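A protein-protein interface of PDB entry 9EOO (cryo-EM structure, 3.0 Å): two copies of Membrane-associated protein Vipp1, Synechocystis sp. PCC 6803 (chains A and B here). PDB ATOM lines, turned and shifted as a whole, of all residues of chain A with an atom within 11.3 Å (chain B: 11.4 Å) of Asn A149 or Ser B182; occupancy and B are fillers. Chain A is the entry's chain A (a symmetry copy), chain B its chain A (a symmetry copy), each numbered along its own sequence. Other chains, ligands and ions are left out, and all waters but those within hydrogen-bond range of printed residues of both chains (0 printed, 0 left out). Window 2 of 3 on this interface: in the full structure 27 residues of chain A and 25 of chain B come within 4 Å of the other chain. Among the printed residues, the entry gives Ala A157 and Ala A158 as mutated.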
ATOM      1  N   ALA A 141       1.860 -10.878   3.444  1.00  0.00           N
ATOM      2  CA  ALA A 141       1.913 -11.549   2.152  1.00  0.00           C
ATOM      3  C   ALA A 141       3.217 -11.291   1.410  1.00  0.00           C
ATOM      4  O   ALA A 141       3.891 -12.226   0.966  1.00  0.00           O
ATOM      5  CB  ALA A 141       0.734 -11.096   1.303  1.00  0.00           C
ATOM      6  N   ARG A 142       3.588 -10.022   1.275  1.00  0.00           N
ATOM      7  CA  ARG A 142       4.839  -9.641   0.632  1.00  0.00           C
ATOM      8  C   ARG A 142       6.073 -10.225   1.298  1.00  0.00           C
ATOM      9  O   ARG A 142       7.051 -10.541   0.615  1.00  0.00           O
ATOM     10  CB  ARG A 142       4.939  -8.126   0.625  1.00  0.00           C
ATOM     11  CG  ARG A 142       4.038  -7.452  -0.357  1.00  0.00           C
ATOM     12  CD  ARG A 142       4.145  -5.962  -0.223  1.00  0.00           C
ATOM     13  NE  ARG A 142       3.513  -5.268  -1.333  1.00  0.00           N
ATOM     14  CZ  ARG A 142       3.899  -4.089  -1.794  1.00  0.00           C
ATOM     15  NH1 ARG A 142       4.920  -3.442  -1.264  1.00  0.00           N
ATOM     16  NH2 ARG A 142       3.265  -3.558  -2.834  1.00  0.00           N
ATOM     17  N   ALA A 143       6.062 -10.375   2.617  1.00  0.00           N
ATOM     18  CA  ALA A 143       7.210 -10.957   3.299  1.00  0.00           C
ATOM     19  C   ALA A 143       7.353 -12.453   3.064  1.00  0.00           C
ATOM     20  O   ALA A 143       8.470 -12.977   3.111  1.00  0.00           O
ATOM     21  CB  ALA A 143       7.107 -10.684   4.792  1.00  0.00           C
ATOM     22  N   LYS A 144       6.255 -13.156   2.829  1.00  0.00           N
ATOM     23  CA  LYS A 144       6.340 -14.560   2.445  1.00  0.00           C
ATOM     24  C   LYS A 144       6.813 -14.745   1.010  1.00  0.00           C
ATOM     25  O   LYS A 144       7.634 -15.624   0.731  1.00  0.00           O
ATOM     26  CB  LYS A 144       4.986 -15.217   2.640  1.00  0.00           C
ATOM     27  CG  LYS A 144       4.673 -15.524   4.086  1.00  0.00           C
ATOM     28  CD  LYS A 144       3.231 -15.951   4.285  1.00  0.00           C
ATOM     29  CE  LYS A 144       2.854 -17.137   3.408  1.00  0.00           C
ATOM     30  NZ  LYS A 144       3.602 -18.364   3.791  1.00  0.00           N
ATOM     31  N   ALA A 145       6.306 -13.934   0.088  1.00  0.00           N
ATOM     32  CA  ALA A 145       6.767 -13.985  -1.293  1.00  0.00           C
ATOM     33  C   ALA A 145       8.251 -13.683  -1.426  1.00  0.00           C
ATOM     34  O   ALA A 145       8.983 -14.399  -2.117  1.00  0.00           O
ATOM     35  CB  ALA A 145       5.953 -13.014  -2.136  1.00  0.00           C
ATOM     36  N   ALA A 146       8.718 -12.628  -0.771  1.00  0.00           N
ATOM     37  CA  ALA A 146      10.122 -12.258  -0.872  1.00  0.00           C
ATOM     38  C   ALA A 146      11.052 -13.320  -0.309  1.00  0.00           C
ATOM     39  O   ALA A 146      12.162 -13.506  -0.816  1.00  0.00           O
ATOM     40  CB  ALA A 146      10.351 -10.945  -0.138  1.00  0.00           C
ATOM     41  N   LYS A 147      10.623 -14.019   0.730  1.00  0.00           N
ATOM     42  CA  LYS A 147      11.440 -15.052   1.345  1.00  0.00           C
ATOM     43  C   LYS A 147      11.501 -16.331   0.521  1.00  0.00           C
ATOM     44  O   LYS A 147      12.532 -17.010   0.498  1.00  0.00           O
ATOM     45  CB  LYS A 147      10.896 -15.329   2.737  1.00  0.00           C
ATOM     46  CG  LYS A 147      11.683 -16.300   3.549  1.00  0.00           C
ATOM     47  CD  LYS A 147      11.470 -16.039   5.032  1.00  0.00           C
ATOM     48  CE  LYS A 147       9.999 -15.947   5.401  1.00  0.00           C
ATOM     49  NZ  LYS A 147       9.808 -15.600   6.835  1.00  0.00           N
ATOM     50  N   ALA A 148      10.409 -16.677  -0.151  1.00  0.00           N
ATOM     51  CA  ALA A 148      10.419 -17.786  -1.096  1.00  0.00           C
ATOM     52  C   ALA A 148      11.336 -17.541  -2.287  1.00  0.00           C
ATOM     53  O   ALA A 148      12.071 -18.441  -2.707  1.00  0.00           O
ATOM     54  CB  ALA A 148       9.002 -18.045  -1.584  1.00  0.00           C
ATOM     55  N   ASN A 149      11.308 -16.334  -2.845  1.00  0.00           N
ATOM     56  CA  ASN A 149      12.220 -15.980  -3.926  1.00  0.00           C
ATOM     57  C   ASN A 149      13.679 -15.918  -3.500  1.00  0.00           C
ATOM     58  O   ASN A 149      14.565 -16.208  -4.309  1.00  0.00           O
ATOM     59  CB  ASN A 149      11.806 -14.640  -4.510  1.00  0.00           C
ATOM     60  CG  ASN A 149      10.612 -14.755  -5.404  1.00  0.00           C
ATOM     61  OD1 ASN A 149       9.479 -14.518  -4.992  1.00  0.00           O
ATOM     62  ND2 ASN A 149      10.857 -15.129  -6.645  1.00  0.00           N
ATOM     63  N   ALA A 150      13.959 -15.546  -2.260  1.00  0.00           N
ATOM     64  CA  ALA A 150      15.337 -15.567  -1.788  1.00  0.00           C
ATOM     65  C   ALA A 150      15.913 -16.975  -1.739  1.00  0.00           C
ATOM     66  O   ALA A 150      17.078 -17.186  -2.095  1.00  0.00           O
ATOM     67  CB  ALA A 150      15.415 -14.925  -0.410  1.00  0.00           C
ATOM     68  N   GLU A 151      15.122 -17.949  -1.302  1.00  0.00           N
ATOM     69  CA  GLU A 151      15.572 -19.338  -1.297  1.00  0.00           C
ATOM     70  C   GLU A 151      15.760 -19.898  -2.697  1.00  0.00           C
ATOM     71  O   GLU A 151      16.692 -20.671  -2.942  1.00  0.00           O
ATOM     72  CB  GLU A 151      14.571 -20.186  -0.528  1.00  0.00           C
ATOM     73  CG  GLU A 151      14.616 -19.970   0.963  1.00  0.00           C
ATOM     74  CD  GLU A 151      13.652 -20.861   1.711  1.00  0.00           C
ATOM     75  OE1 GLU A 151      12.515 -21.048   1.229  1.00  0.00           O
ATOM     76  OE2 GLU A 151      14.028 -21.375   2.786  1.00  0.00           O
ATOM     77  N   LEU A 152      14.888 -19.531  -3.630  1.00  0.00           N
ATOM     78  CA  LEU A 152      15.065 -19.932  -5.019  1.00  0.00           C
ATOM     79  C   LEU A 152      16.350 -19.388  -5.627  1.00  0.00           C
ATOM     80  O   LEU A 152      17.127 -20.137  -6.229  1.00  0.00           O
ATOM     81  CB  LEU A 152      13.870 -19.463  -5.833  1.00  0.00           C
ATOM     82  CG  LEU A 152      13.934 -19.767  -7.319  1.00  0.00           C
ATOM     83  CD1 LEU A 152      12.588 -20.108  -7.830  1.00  0.00           C
ATOM     84  CD2 LEU A 152      14.446 -18.576  -8.061  1.00  0.00           C
ATOM     85  N   GLN A 153      16.598 -18.092  -5.478  1.00  0.00           N
ATOM     86  CA  GLN A 153      17.793 -17.503  -6.064  1.00  0.00           C
ATOM     87  C   GLN A 153      19.071 -18.040  -5.435  1.00  0.00           C
ATOM     88  O   GLN A 153      20.113 -18.087  -6.094  1.00  0.00           O
ATOM     89  CB  GLN A 153      17.737 -15.987  -5.921  1.00  0.00           C
ATOM     90  CG  GLN A 153      16.647 -15.335  -6.743  1.00  0.00           C
ATOM     91  CD  GLN A 153      16.829 -15.533  -8.229  1.00  0.00           C
ATOM     92  OE1 GLN A 153      17.941 -15.746  -8.706  1.00  0.00           O
ATOM     93  NE2 GLN A 153      15.729 -15.471  -8.969  1.00  0.00           N
ATOM     94  N   GLN A 154      19.013 -18.448  -4.173  1.00  0.00           N
ATOM     95  CA  GLN A 154      20.145 -19.118  -3.549  1.00  0.00           C
ATOM     96  C   GLN A 154      20.376 -20.516  -4.103  1.00  0.00           C
ATOM     97  O   GLN A 154      21.523 -20.972  -4.176  1.00  0.00           O
ATOM     98  CB  GLN A 154      19.919 -19.184  -2.049  1.00  0.00           C
ATOM     99  CG  GLN A 154      21.024 -19.831  -1.280  1.00  0.00           C
ATOM    100  CD  GLN A 154      20.787 -19.765   0.212  1.00  0.00           C
ATOM    101  OE1 GLN A 154      19.726 -19.339   0.662  1.00  0.00           O
ATOM    102  NE2 GLN A 154      21.777 -20.186   0.987  1.00  0.00           N
ATOM    103  N   THR A 155      19.310 -21.210  -4.484  1.00  0.00           N
ATOM    104  CA  THR A 155      19.438 -22.545  -5.054  1.00  0.00           C
ATOM    105  C   THR A 155      20.073 -22.521  -6.438  1.00  0.00           C
ATOM    106  O   THR A 155      20.940 -23.348  -6.745  1.00  0.00           O
ATOM    107  CB  THR A 155      18.062 -23.203  -5.107  1.00  0.00           C
ATOM    108  OG1 THR A 155      17.552 -23.344  -3.779  1.00  0.00           O
ATOM    109  CG2 THR A 155      18.136 -24.557  -5.746  1.00  0.00           C
ATOM    110  N   LEU A 156      19.655 -21.586  -7.285  1.00  0.00           N
ATOM    111  CA  LEU A 156      20.240 -21.434  -8.611  1.00  0.00           C
ATOM    112  C   LEU A 156      21.712 -21.052  -8.577  1.00  0.00           C
ATOM    113  O   LEU A 156      22.473 -21.448  -9.465  1.00  0.00           O
ATOM    114  CB  LEU A 156      19.465 -20.378  -9.383  1.00  0.00           C
ATOM    115  CG  LEU A 156      18.266 -20.877 -10.167  1.00  0.00           C
ATOM    116  CD1 LEU A 156      17.343 -21.556  -9.238  1.00  0.00           C
ATOM    117  CD2 LEU A 156      17.552 -19.742 -10.832  1.00  0.00           C
ATOM    118  N   ALA A 157      22.133 -20.289  -7.577  1.00  0.00           N
ATOM    119  CA  ALA A 157      23.545 -19.951  -7.451  1.00  0.00           C
ATOM    120  C   ALA A 157      24.402 -21.161  -7.097  1.00  0.00           C
ATOM    121  O   ALA A 157      25.449 -21.390  -7.711  1.00  0.00           O
ATOM    122  CB  ALA A 157      23.710 -18.865  -6.397  1.00  0.00           C
ATOM    123  N   ALA A 158      23.977 -21.949  -6.114  1.00  0.00           N
ATOM    124  CA  ALA A 158      24.745 -23.127  -5.727  1.00  0.00           C
ATOM    125  C   ALA A 158      24.834 -24.155  -6.850  1.00  0.00           C
ATOM    126  O   ALA A 158      25.864 -24.823  -7.006  1.00  0.00           O
ATOM    127  CB  ALA A 158      24.129 -23.757  -4.484  1.00  0.00           C
ATOM    128  N   ASN B 173       9.231  -1.174   6.981  1.00  0.00           N
ATOM    129  CA  ASN B 173      10.422  -0.905   6.185  1.00  0.00           C
ATOM    130  C   ASN B 173      11.313  -2.132   6.014  1.00  0.00           C
ATOM    131  O   ASN B 173      11.870  -2.354   4.935  1.00  0.00           O
ATOM    132  CB  ASN B 173      11.209   0.229   6.829  1.00  0.00           C
ATOM    133  CG  ASN B 173      10.463   1.539   6.796  1.00  0.00           C
ATOM    134  OD1 ASN B 173       9.668   1.795   5.894  1.00  0.00           O
ATOM    135  ND2 ASN B 173      10.706   2.375   7.791  1.00  0.00           N
ATOM    136  N   LYS B 174      11.460  -2.940   7.060  1.00  0.00           N
ATOM    137  CA  LYS B 174      12.154  -4.219   6.928  1.00  0.00           C
ATOM    138  C   LYS B 174      11.549  -5.119   5.860  1.00  0.00           C
ATOM    139  O   LYS B 174      12.277  -5.801   5.131  1.00  0.00           O
ATOM    140  CB  LYS B 174      12.148  -4.955   8.254  1.00  0.00           C
ATOM    141  CG  LYS B 174      13.138  -4.464   9.254  1.00  0.00           C
ATOM    142  CD  LYS B 174      13.307  -5.490  10.341  1.00  0.00           C
ATOM    143  CE  LYS B 174      14.340  -5.081  11.351  1.00  0.00           C
ATOM    144  NZ  LYS B 174      14.612  -6.186  12.300  1.00  0.00           N
ATOM    145  N   VAL B 175      10.227  -5.146   5.756  1.00  0.00           N
ATOM    146  CA  VAL B 175       9.581  -5.957   4.732  1.00  0.00           C
ATOM    147  C   VAL B 175       9.876  -5.429   3.337  1.00  0.00           C
ATOM    148  O   VAL B 175      10.146  -6.200   2.410  1.00  0.00           O
ATOM    149  CB  VAL B 175       8.071  -6.010   5.007  1.00  0.00           C
ATOM    150  CG1 VAL B 175       7.340  -6.656   3.868  1.00  0.00           C
ATOM    151  CG2 VAL B 175       7.816  -6.751   6.282  1.00  0.00           C
ATOM    152  N   LEU B 176       9.829  -4.117   3.166  1.00  0.00           N
ATOM    153  CA  LEU B 176      10.100  -3.517   1.870  1.00  0.00           C
ATOM    154  C   LEU B 176      11.556  -3.651   1.452  1.00  0.00           C
ATOM    155  O   LEU B 176      11.852  -3.692   0.254  1.00  0.00           O
ATOM    156  CB  LEU B 176       9.690  -2.056   1.911  1.00  0.00           C
ATOM    157  CG  LEU B 176       8.274  -1.759   1.437  1.00  0.00           C
ATOM    158  CD1 LEU B 176       7.315  -2.689   2.087  1.00  0.00           C
ATOM    159  CD2 LEU B 176       7.903  -0.356   1.786  1.00  0.00           C
ATOM    160  N   ASP B 177      12.473  -3.716   2.412  1.00  0.00           N
ATOM    161  CA  ASP B 177      13.866  -4.009   2.094  1.00  0.00           C
ATOM    162  C   ASP B 177      14.072  -5.432   1.586  1.00  0.00           C
ATOM    163  O   ASP B 177      14.821  -5.650   0.631  1.00  0.00           O
ATOM    164  CB  ASP B 177      14.724  -3.771   3.328  1.00  0.00           C
ATOM    165  CG  ASP B 177      14.784  -2.315   3.726  1.00  0.00           C
ATOM    166  OD1 ASP B 177      14.426  -1.455   2.893  1.00  0.00           O
ATOM    167  OD2 ASP B 177      15.191  -2.025   4.869  1.00  0.00           O
ATOM    168  N   MET B 178      13.410  -6.408   2.201  1.00  0.00           N
ATOM    169  CA  MET B 178      13.499  -7.787   1.732  1.00  0.00           C
ATOM    170  C   MET B 178      12.920  -7.955   0.335  1.00  0.00           C
ATOM    171  O   MET B 178      13.520  -8.602  -0.528  1.00  0.00           O
ATOM    172  CB  MET B 178      12.770  -8.706   2.704  1.00  0.00           C
ATOM    173  CG  MET B 178      13.395  -8.801   4.065  1.00  0.00           C
ATOM    174  SD  MET B 178      12.302  -9.649   5.222  1.00  0.00           S
ATOM    175  CE  MET B 178      13.152  -9.366   6.768  1.00  0.00           C
ATOM    176  N   GLU B 179      11.747  -7.383   0.101  1.00  0.00           N
ATOM    177  CA  GLU B 179      11.090  -7.502  -1.193  1.00  0.00           C
ATOM    178  C   GLU B 179      11.937  -6.948  -2.334  1.00  0.00           C
ATOM    179  O   GLU B 179      12.029  -7.565  -3.402  1.00  0.00           O
ATOM    180  CB  GLU B 179       9.740  -6.795  -1.132  1.00  0.00           C
ATOM    181  CG  GLU B 179       9.005  -6.703  -2.440  1.00  0.00           C
ATOM    182  CD  GLU B 179       7.686  -5.977  -2.310  1.00  0.00           C
ATOM    183  OE1 GLU B 179       6.757  -6.545  -1.703  1.00  0.00           O
ATOM    184  OE2 GLU B 179       7.576  -4.841  -2.810  1.00  0.00           O
ATOM    185  N   ALA B 180      12.562  -5.793  -2.135  1.00  0.00           N
ATOM    186  CA  ALA B 180      13.406  -5.211  -3.173  1.00  0.00           C
ATOM    187  C   ALA B 180      14.687  -6.001  -3.399  1.00  0.00           C
ATOM    188  O   ALA B 180      15.149  -6.132  -4.536  1.00  0.00           O
ATOM    189  CB  ALA B 180      13.735  -3.775  -2.802  1.00  0.00           C
ATOM    190  N   THR B 181      15.277  -6.533  -2.333  1.00  0.00           N
ATOM    191  CA  THR B 181      16.491  -7.329  -2.466  1.00  0.00           C
ATOM    192  C   THR B 181      16.263  -8.609  -3.262  1.00  0.00           C
ATOM    193  O   THR B 181      17.097  -8.992  -4.090  1.00  0.00           O
ATOM    194  CB  THR B 181      17.024  -7.658  -1.079  1.00  0.00           C
ATOM    195  OG1 THR B 181      17.395  -6.451  -0.410  1.00  0.00           O
ATOM    196  CG2 THR B 181      18.205  -8.568  -1.161  1.00  0.00           C
ATOM    197  N   SER B 182      15.148  -9.284  -3.018  1.00  0.00           N
ATOM    198  CA  SER B 182      14.779 -10.469  -3.787  1.00  0.00           C
ATOM    199  C   SER B 182      14.492 -10.154  -5.249  1.00  0.00           C
ATOM    200  O   SER B 182      14.977 -10.846  -6.150  1.00  0.00           O
ATOM    201  CB  SER B 182      13.565 -11.127  -3.144  1.00  0.00           C
ATOM    202  OG  SER B 182      13.131 -12.239  -3.900  1.00  0.00           O
ATOM    203  N   GLN B 183      13.708  -9.114  -5.507  1.00  0.00           N
ATOM    204  CA  GLN B 183      13.298  -8.798  -6.869  1.00  0.00           C
ATOM    205  C   GLN B 183      14.456  -8.347  -7.745  1.00  0.00           C
ATOM    206  O   GLN B 183      14.501  -8.680  -8.936  1.00  0.00           O
ATOM    207  CB  GLN B 183      12.226  -7.716  -6.834  1.00  0.00           C
ATOM    208  CG  GLN B 183      10.874  -8.207  -6.382  1.00  0.00           C
ATOM    209  CD  GLN B 183       9.824  -7.114  -6.319  1.00  0.00           C
ATOM    210  OE1 GLN B 183       8.710  -7.345  -5.854  1.00  0.00           O
ATOM    211  NE2 GLN B 183      10.170  -5.918  -6.786  1.00  0.00           N
ATOM    212  N   ALA B 184      15.396  -7.589  -7.195  1.00  0.00           N
ATOM    213  CA  ALA B 184      16.539  -7.156  -7.988  1.00  0.00           C
ATOM    214  C   ALA B 184      17.454  -8.311  -8.370  1.00  0.00           C
ATOM    215  O   ALA B 184      17.891  -8.404  -9.523  1.00  0.00           O
ATOM    216  CB  ALA B 184      17.324  -6.110  -7.215  1.00  0.00           C
ATOM    217  N   ALA B 185      17.751  -9.200  -7.430  1.00  0.00           N
ATOM    218  CA  ALA B 185      18.574 -10.360  -7.749  1.00  0.00           C
ATOM    219  C   ALA B 185      17.904 -11.286  -8.753  1.00  0.00           C
ATOM    220  O   ALA B 185      18.572 -11.867  -9.614  1.00  0.00           O
ATOM    221  CB  ALA B 185      18.899 -11.125  -6.472  1.00  0.00           C
ATOM    222  N   GLY B 186      16.586 -11.434  -8.664  1.00  0.00           N
ATOM    223  CA  GLY B 186      15.875 -12.230  -9.648  1.00  0.00           C
ATOM    224  C   GLY B 186      15.768 -11.566 -11.003  1.00  0.00           C
ATOM    225  O   GLY B 186      15.872 -12.225 -12.040  1.00  0.00           O
ATOM    226  N   GLU B 187      15.561 -10.254 -11.018  1.00  0.00           N
ATOM    227  CA  GLU B 187      15.480  -9.534 -12.282  1.00  0.00           C
ATOM    228  C   GLU B 187      16.798  -9.586 -13.036  1.00  0.00           C
ATOM    229  O   GLU B 187      16.820  -9.770 -14.255  1.00  0.00           O
ATOM    230  CB  GLU B 187      15.081  -8.086 -12.014  1.00  0.00           C
ATOM    231  CG  GLU B 187      15.077  -7.197 -13.228  1.00  0.00           C
ATOM    232  CD  GLU B 187      14.726  -5.765 -12.885  1.00  0.00           C
ATOM    233  OE1 GLU B 187      13.821  -5.560 -12.051  1.00  0.00           O
ATOM    234  OE2 GLU B 187      15.360  -4.844 -13.444  1.00  0.00           O
ATOM    235  N   LEU B 188      17.908  -9.413 -12.325  1.00  0.00           N
ATOM    236  CA  LEU B 188      19.204  -9.376 -12.985  1.00  0.00           C
ATOM    237  C   LEU B 188      19.588 -10.737 -13.546  1.00  0.00           C
ATOM    238  O   LEU B 188      20.204 -10.824 -14.616  1.00  0.00           O
ATOM    239  CB  LEU B 188      20.246  -8.891 -11.987  1.00  0.00           C
ATOM    240  CG  LEU B 188      21.547  -8.339 -12.522  1.00  0.00           C
ATOM    241  CD1 LEU B 188      21.292  -7.006 -13.157  1.00  0.00           C
ATOM    242  CD2 LEU B 188      22.485  -8.188 -11.372  1.00  0.00           C
ATOM    243  N   ALA B 189      19.235 -11.810 -12.840  1.00  0.00           N
ATOM    244  CA  ALA B 189      19.421 -13.155 -13.365  1.00  0.00           C
ATOM    245  C   ALA B 189      18.492 -13.463 -14.530  1.00  0.00           C
ATOM    246  O   ALA B 189      18.727 -14.435 -15.255  1.00  0.00           O
ATOM    247  CB  ALA B 189      19.213 -14.182 -12.257  1.00  0.00           C
ATOM    248  N   GLY B 190      17.452 -12.654 -14.729  1.00  0.00           N
ATOM    249  CA  GLY B 190      16.593 -12.818 -15.884  1.00  0.00           C
ATOM    250  C   GLY B 190      17.232 -12.367 -17.174  1.00  0.00           C
ATOM    251  O   GLY B 190      16.761 -12.734 -18.254  1.00  0.00           O
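The guanidinium group (NH1) of Arg A142 lies within salt-bridge range of the side-chain carboxylate (OE2) of Glu B179, 3.4 Å away. OG of Ser B182 sits at hydrogen-bond distance from O of Ala A146 (3.5 Å).
OD1 of Asn A149 lies close to O of Ala A145, at 2.9 Å.
Among the printed residues, merely in contact across the chains: Ala A146 with Met B178 (3.96 Å), Ala A146 with Glu B179 (3.7 Å), Asn A149 with Ser B182 (2.8 Å), Ala A150 with Ser B182 (3.8 Å) and Gln A153 with Gly B186 (3.3 Å).
Of the printed residues of chain B, Arg A142 touches Glu B179 (3.1 Å). No residue of chain B comes within 4 Å of Ala A145. Ala A146 touches three residues of chain B. No residue of chain B comes within 4 Å of Ala A148. Of chain B, only Ser B182 (2.8 Å) comes within 4 Å of Asn A149. Of chain B, only Ser B182 (3.8 Å) comes within 4 Å of Ala A150. Glu A151 touches none of the printed residues of chain B. No residue of chain B comes within 4 Å of Leu A152. Gln A153 touches just one residue of chain B: Gly B186 (3.3 Å). Asp B177 touches none of the printed residues of chain A. Of the printed residues of chain A, Met B178 touches Ala A146 (3.96 Å). Printed residues of chain A within 4 Å of Glu B179: Arg A142 and Ala A146. No residue of chain A comes within 4 Å of Thr B181. Of chain A, only Ala A146, Asn A149 and Ala A150 come within 4 Å of Ser B182. No residue of chain A comes within 4 Å of Gln B183. Of chain A, only Gln A153 (3.3 Å) comes within 4 Å of Gly B186. The nearest residue of chain A that does not touch Ser B182 is Gln A153 (4.8 Å).
Of the 18 printed residues of chain A, 5 touch a printed residue of chain B. Printed residues of chain A that touch a printed residue of chain B: Arg A142, Ala A146, Asn A149, Ala A150 and Gln A153. Among the printed residues, Asp or Glu carboxylates within 4 Å of a Lys or Arg side-chain nitrogen of the other chain: Arg A142 with Glu B179.
No position is printed for both chains.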
